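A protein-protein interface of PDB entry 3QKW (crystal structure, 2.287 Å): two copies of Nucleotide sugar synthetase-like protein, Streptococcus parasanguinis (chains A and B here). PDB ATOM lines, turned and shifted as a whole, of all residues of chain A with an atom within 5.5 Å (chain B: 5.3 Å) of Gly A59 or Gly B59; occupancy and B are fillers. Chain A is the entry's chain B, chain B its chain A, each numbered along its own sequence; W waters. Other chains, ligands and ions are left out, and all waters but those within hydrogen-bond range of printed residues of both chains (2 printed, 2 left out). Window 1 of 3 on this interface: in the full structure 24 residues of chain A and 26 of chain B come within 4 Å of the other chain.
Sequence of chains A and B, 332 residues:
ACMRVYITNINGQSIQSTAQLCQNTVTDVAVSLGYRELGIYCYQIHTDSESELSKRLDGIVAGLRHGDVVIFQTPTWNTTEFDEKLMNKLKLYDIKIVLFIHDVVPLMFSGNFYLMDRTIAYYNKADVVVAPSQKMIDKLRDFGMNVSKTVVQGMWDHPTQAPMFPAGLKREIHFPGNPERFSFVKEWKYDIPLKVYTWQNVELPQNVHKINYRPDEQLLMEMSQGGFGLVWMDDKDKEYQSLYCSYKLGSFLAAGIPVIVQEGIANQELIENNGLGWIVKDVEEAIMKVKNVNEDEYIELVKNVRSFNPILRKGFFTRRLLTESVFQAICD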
ATOM      1  N   GLY A  39     -21.618   1.070   2.308  1.00  0.00           N
ATOM      2  CA  GLY A  39     -20.235   0.778   1.953  1.00  0.00           C
ATOM      3  C   GLY A  39     -19.630   1.873   1.099  1.00  0.00           C
ATOM      4  O   GLY A  39     -20.248   2.320   0.114  1.00  0.00           O
ATOM      5  N   SER A  54     -20.896  12.767  -8.099  1.00  0.00           N
ATOM      6  CA  SER A  54     -22.284  12.875  -7.636  1.00  0.00           C
ATOM      7  C   SER A  54     -23.077  11.574  -7.832  1.00  0.00           C
ATOM      8  O   SER A  54     -23.881  11.198  -6.981  1.00  0.00           O
ATOM      9  CB  SER A  54     -22.999  14.054  -8.302  1.00  0.00           C
ATOM     10  OG  SER A  54     -24.402  14.001  -8.077  1.00  0.00           O
ATOM     11  N   LYS A  55     -22.841  10.875  -8.937  1.00  0.00           N
ATOM     12  CA  LYS A  55     -23.571   9.632  -9.179  1.00  0.00           C
ATOM     13  C   LYS A  55     -23.006   8.397  -8.445  1.00  0.00           C
ATOM     14  O   LYS A  55     -23.758   7.458  -8.139  1.00  0.00           O
ATOM     15  CB  LYS A  55     -23.730   9.370 -10.671  1.00  0.00           C
ATOM     16  CG  LYS A  55     -24.500  10.489 -11.375  1.00  0.00           C
ATOM     17  CD  LYS A  55     -24.942  10.096 -12.771  1.00  0.00           C
ATOM     18  CE  LYS A  55     -25.785  11.203 -13.391  1.00  0.00           C
ATOM     19  NZ  LYS A  55     -26.286  10.830 -14.723  1.00  0.00           N
ATOM     20  N   ARG A  56     -21.702   8.394  -8.175  1.00  0.00           N
ATOM     21  CA  ARG A  56     -21.091   7.330  -7.365  1.00  0.00           C
ATOM     22  C   ARG A  56     -21.675   7.403  -5.962  1.00  0.00           C
ATOM     23  O   ARG A  56     -22.096   6.392  -5.391  1.00  0.00           O
ATOM     24  CB  ARG A  56     -19.585   7.511  -7.267  1.00  0.00           C
ATOM     25  CG  ARG A  56     -18.866   6.442  -6.450  1.00  0.00           C
ATOM     26  CD  ARG A  56     -17.401   6.815  -6.236  1.00  0.00           C
ATOM     27  NE  ARG A  56     -16.646   6.941  -7.492  1.00  0.00           N
ATOM     28  CZ  ARG A  56     -16.077   5.912  -8.114  1.00  0.00           C
ATOM     29  NH1 ARG A  56     -16.197   4.693  -7.607  1.00  0.00           N
ATOM     30  NH2 ARG A  56     -15.391   6.094  -9.235  1.00  0.00           N
ATOM     31  N   LEU A  57     -21.695   8.619  -5.420  1.00  0.00           N
ATOM     32  CA  LEU A  57     -22.379   8.908  -4.167  1.00  0.00           C
ATOM     33  C   LEU A  57     -23.865   8.497  -4.189  1.00  0.00           C
ATOM     34  O   LEU A  57     -24.358   7.909  -3.229  1.00  0.00           O
ATOM     35  CB  LEU A  57     -22.227  10.387  -3.825  1.00  0.00           C
ATOM     36  CG  LEU A  57     -20.799  10.808  -3.481  1.00  0.00           C
ATOM     37  CD1 LEU A  57     -20.650  12.319  -3.509  1.00  0.00           C
ATOM     38  CD2 LEU A  57     -20.390  10.241  -2.123  1.00  0.00           C
ATOM     39  N   ASP A  58     -24.566   8.793  -5.280  1.00  0.00           N
ATOM     40  CA  ASP A  58     -25.959   8.379  -5.443  1.00  0.00           C
ATOM     41  C   ASP A  58     -26.066   6.860  -5.395  1.00  0.00           C
ATOM     42  O   ASP A  58     -27.078   6.304  -4.959  1.00  0.00           O
ATOM     43  CB  ASP A  58     -26.548   8.868  -6.772  1.00  0.00           C
ATOM     44  CG  ASP A  58     -26.998  10.329  -6.738  1.00  0.00           C
ATOM     45  OD1 ASP A  58     -26.889  10.971  -5.676  1.00  0.00           O
ATOM     46  OD2 ASP A  58     -27.485  10.825  -7.790  1.00  0.00           O
ATOM     47  N   GLY A  59     -25.030   6.181  -5.871  1.00  0.00           N
ATOM     48  CA  GLY A  59     -25.048   4.730  -5.849  1.00  0.00           C
ATOM     49  C   GLY A  59     -24.866   4.202  -4.432  1.00  0.00           C
ATOM     50  O   GLY A  59     -25.487   3.220  -4.042  1.00  0.00           O
ATOM     51  N   ILE A  60     -23.993   4.859  -3.678  1.00  0.00           N
ATOM     52  CA  ILE A  60     -23.715   4.521  -2.290  1.00  0.00           C
ATOM     53  C   ILE A  60     -24.941   4.699  -1.364  1.00  0.00           C
ATOM     54  O   ILE A  60     -25.202   3.846  -0.515  1.00  0.00           O
ATOM     55  CB  ILE A  60     -22.535   5.356  -1.774  1.00  0.00           C
ATOM     56  CG1 ILE A  60     -21.243   4.922  -2.464  1.00  0.00           C
ATOM     57  CG2 ILE A  60     -22.393   5.236  -0.275  1.00  0.00           C
ATOM     58  CD1 ILE A  60     -20.031   5.718  -2.039  1.00  0.00           C
ATOM     59  N   VAL A  61     -25.685   5.793  -1.542  1.00  0.00           N
ATOM     60  CA  VAL A  61     -26.859   6.078  -0.722  1.00  0.00           C
ATOM     61  C   VAL A  61     -28.201   5.708  -1.376  1.00  0.00           C
ATOM     62  O   VAL A  61     -29.236   6.187  -0.961  1.00  0.00           O
ATOM     63  CB  VAL A  61     -26.914   7.570  -0.287  1.00  0.00           C
ATOM     64  CG1 VAL A  61     -25.625   7.967   0.423  1.00  0.00           C
ATOM     65  CG2 VAL A  61     -27.192   8.484  -1.473  1.00  0.00           C
ATOM     66  N   ALA A  62     -28.189   4.822  -2.361  1.00  0.00           N
ATOM     67  CA  ALA A  62     -29.414   4.508  -3.092  1.00  0.00           C
ATOM     68  C   ALA A  62     -30.539   4.022  -2.202  1.00  0.00           C
ATOM     69  O   ALA A  62     -31.708   4.158  -2.553  1.00  0.00           O
ATOM     70  CB  ALA A  62     -29.145   3.464  -4.177  1.00  0.00           C
ATOM     71  N   GLY B  39     -28.367  -1.533  -1.613  1.00  0.00           N
ATOM     72  CA  GLY B  39     -29.420  -0.659  -2.115  1.00  0.00           C
ATOM     73  C   GLY B  39     -29.288  -0.214  -3.569  1.00  0.00           C
ATOM     74  O   GLY B  39     -28.237   0.285  -3.995  1.00  0.00           O
ATOM     75  N   SER B  54     -21.276   3.132 -14.764  1.00  0.00           N
ATOM     76  CA  SER B  54     -20.283   2.217 -14.233  1.00  0.00           C
ATOM     77  C   SER B  54     -19.951   2.572 -12.791  1.00  0.00           C
ATOM     78  O   SER B  54     -19.888   1.704 -11.926  1.00  0.00           O
ATOM     79  CB  SER B  54     -19.025   2.276 -15.091  1.00  0.00           C
ATOM     80  OG  SER B  54     -17.982   1.491 -14.561  1.00  0.00           O
ATOM     81  N   LYS B  55     -19.749   3.857 -12.541  1.00  0.00           N
ATOM     82  CA  LYS B  55     -19.324   4.321 -11.233  1.00  0.00           C
ATOM     83  C   LYS B  55     -20.459   4.421 -10.217  1.00  0.00           C
ATOM     84  O   LYS B  55     -20.221   4.331  -9.011  1.00  0.00           O
ATOM     85  CB  LYS B  55     -18.582   5.636 -11.369  1.00  0.00           C
ATOM     86  CG  LYS B  55     -17.366   5.500 -12.283  1.00  0.00           C
ATOM     87  CD  LYS B  55     -17.021   6.830 -12.874  1.00  0.00           C
ATOM     88  CE  LYS B  55     -15.909   7.469 -12.112  1.00  0.00           C
ATOM     89  NZ  LYS B  55     -14.658   7.493 -12.917  1.00  0.00           N
ATOM     90  N   ARG B  56     -21.685   4.606 -10.705  1.00  0.00           N
ATOM     91  CA  ARG B  56     -22.865   4.474  -9.858  1.00  0.00           C
ATOM     92  C   ARG B  56     -22.935   3.035  -9.344  1.00  0.00           C
ATOM     93  O   ARG B  56     -23.164   2.808  -8.163  1.00  0.00           O
ATOM     94  CB  ARG B  56     -24.144   4.814 -10.617  1.00  0.00           C
ATOM     95  CG  ARG B  56     -25.410   4.705  -9.775  1.00  0.00           C
ATOM     96  CD  ARG B  56     -26.669   4.669 -10.636  1.00  0.00           C
ATOM     97  NE  ARG B  56     -26.785   5.867 -11.476  1.00  0.00           N
ATOM     98  CZ  ARG B  56     -27.326   7.020 -11.084  1.00  0.00           C
ATOM     99  NH1 ARG B  56     -27.818   7.158  -9.850  1.00  0.00           N
ATOM    100  NH2 ARG B  56     -27.393   8.038 -11.931  1.00  0.00           N
ATOM    101  N   LEU B  57     -22.720   2.076 -10.243  1.00  0.00           N
ATOM    102  CA  LEU B  57     -22.616   0.679  -9.858  1.00  0.00           C
ATOM    103  C   LEU B  57     -21.451   0.443  -8.879  1.00  0.00           C
ATOM    104  O   LEU B  57     -21.622  -0.252  -7.874  1.00  0.00           O
ATOM    105  CB  LEU B  57     -22.484  -0.219 -11.092  1.00  0.00           C
ATOM    106  CG  LEU B  57     -23.699  -0.328 -12.014  1.00  0.00           C
ATOM    107  CD1 LEU B  57     -23.370  -1.164 -13.263  1.00  0.00           C
ATOM    108  CD2 LEU B  57     -24.819  -0.954 -11.257  1.00  0.00           C
ATOM    109  N   ASP B  58     -20.274   1.013  -9.159  1.00  0.00           N
ATOM    110  CA  ASP B  58     -19.166   0.910  -8.205  1.00  0.00           C
ATOM    111  C   ASP B  58     -19.605   1.465  -6.852  1.00  0.00           C
ATOM    112  O   ASP B  58     -19.066   1.090  -5.819  1.00  0.00           O
ATOM    113  CB  ASP B  58     -17.907   1.665  -8.658  1.00  0.00           C
ATOM    114  CG  ASP B  58     -17.138   0.954  -9.766  1.00  0.00           C
ATOM    115  OD1 ASP B  58     -17.526  -0.168 -10.143  1.00  0.00           O
ATOM    116  OD2 ASP B  58     -16.124   1.519 -10.238  1.00  0.00           O
ATOM    117  N   GLY B  59     -20.568   2.386  -6.868  1.00  0.00           N
ATOM    118  CA  GLY B  59     -21.068   2.982  -5.647  1.00  0.00           C
ATOM    119  C   GLY B  59     -21.920   1.972  -4.895  1.00  0.00           C
ATOM    120  O   GLY B  59     -21.794   1.799  -3.699  1.00  0.00           O
ATOM    121  N   ILE B  60     -22.790   1.293  -5.625  1.00  0.00           N
ATOM    122  CA  ILE B  60     -23.643   0.275  -5.058  1.00  0.00           C
ATOM    123  C   ILE B  60     -22.868  -0.906  -4.442  1.00  0.00           C
ATOM    124  O   ILE B  60     -23.225  -1.399  -3.384  1.00  0.00           O
ATOM    125  CB  ILE B  60     -24.626  -0.180  -6.115  1.00  0.00           C
ATOM    126  CG1 ILE B  60     -25.548   0.990  -6.458  1.00  0.00           C
ATOM    127  CG2 ILE B  60     -25.437  -1.356  -5.656  1.00  0.00           C
ATOM    128  CD1 ILE B  60     -26.371   0.777  -7.721  1.00  0.00           C
ATOM    129  N   VAL B  61     -21.795  -1.333  -5.090  1.00  0.00           N
ATOM    130  CA  VAL B  61     -21.077  -2.517  -4.642  1.00  0.00           C
ATOM    131  C   VAL B  61     -19.772  -2.171  -3.924  1.00  0.00           C
ATOM    132  O   VAL B  61     -18.928  -3.028  -3.707  1.00  0.00           O
ATOM    133  CB  VAL B  61     -20.813  -3.462  -5.818  1.00  0.00           C
ATOM    134  CG1 VAL B  61     -22.104  -3.687  -6.559  1.00  0.00           C
ATOM    135  CG2 VAL B  61     -19.762  -2.877  -6.766  1.00  0.00           C
ATOM    136  N   ALA B  62     -19.622  -0.909  -3.539  1.00  0.00           N
ATOM    137  CA  ALA B  62     -18.392  -0.455  -2.904  1.00  0.00           C
ATOM    138  C   ALA B  62     -17.955  -1.327  -1.730  1.00  0.00           C
ATOM    139  O   ALA B  62     -16.754  -1.463  -1.452  1.00  0.00           O
ATOM    140  CB  ALA B  62     -18.549   0.987  -2.451  1.00  0.00           C
HETATM  141  O   HOH W   1     -17.156   3.086  -5.214  1.00  0.00           O
HETATM  142  O   HOH W   2     -22.173   1.314  -1.071  1.00  0.00           O
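Ala B62 touches Gly A39.
Lys A55 touches Arg B56.
NH2 of Arg A56 touches CE of Lys B55, at 3.2 Å.
CB of Asp B58 touches NH1 of Arg A56, 3.6 Å away.
CA of Gly B59 touches O of Arg A56, at 3.6 Å.
Asp A58 touches Arg B56.
Gly A59 touches Arg B56.
C of Gly B59 touches C of Gly A59, at 3.7 Å.
Gly A59 touches Ile B60 (O to CG1, 3.3 Å).
Ile A60 touches Gly B59 (CG1 to O, 3.4 Å).
Gly A59 touches just these residues of chain B: Arg B56 (3.5 Å), Gly B59 (3.7 Å) and Ile B60 (3.3 Å).
Of chain A, only Arg A56 (3.6 Å), Gly A59 (3.7 Å) and Ile A60 (3.4 Å) come within 4 Å of Gly B59.
Of the printed residues of chain A, Ile B60 touches Gly A59.
Printed residues of chain A within 4 Å of Gly B39: Ala A62 (3.3 Å).
Printed residues of chain B within 4 Å of Ala A62: Gly B39 (3.3 Å).
Printed residues of chain B within 4 Å of Asp A58: Arg B56.
The nearest residue of chain B that does not touch Gly A59 is Gly B39 (4.02 Å).
Of the 10 printed residues of chain A, 7 touch a printed residue of chain B.
Hydrophobic or aromatic side chains of chain A within 4 Å of the printed part of chain B: Ile A60 and Ala A62.
Along chain A the printed residues that touch a printed residue of chain B span positions 39 to 62.
Printed residues of chain B that touch a printed residue of chain A: Gly B39, Lys B55, Arg B56, Asp B58, Gly B59, Ile B60 and Ala B62.
Hydrophobic or aromatic side chains of chain B within 4 Å of the printed part of chain A: Ile B60 and Ala B62.
Among the printed residues, 11 pairs touch across the chains.
Among the printed residues, no Asp or Glu carboxylate lies within 4 Å of a Lys or Arg side-chain nitrogen of the other chain.
Gly A39 touches Ala B62, and with the chains exchanged Ala A62 touches Gly B39.
Arg A56 touches Asp B58, and with the chains exchanged Asp A58 touches Arg B56.
Arg A56 touches Gly B59, and with the chains exchanged Gly A59 touches Arg B56.
Gly A59 touches Ile B60, and with the chains exchanged Ile A60 touches Gly B59.
10 positions are printed for both chains.
Water W2 lies within hydrogen-bond range of the backbone carbonyl oxygen (O) of Gly A39 (2.5 Å) and the backbone carbonyl oxygen (O) of Gly B59 (2.7 Å).
Water W1 bridges the backbone carbonyl oxygen of Asp B58 (2.8 Å) and the guanidinium group of Arg A56 (3.0 Å).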
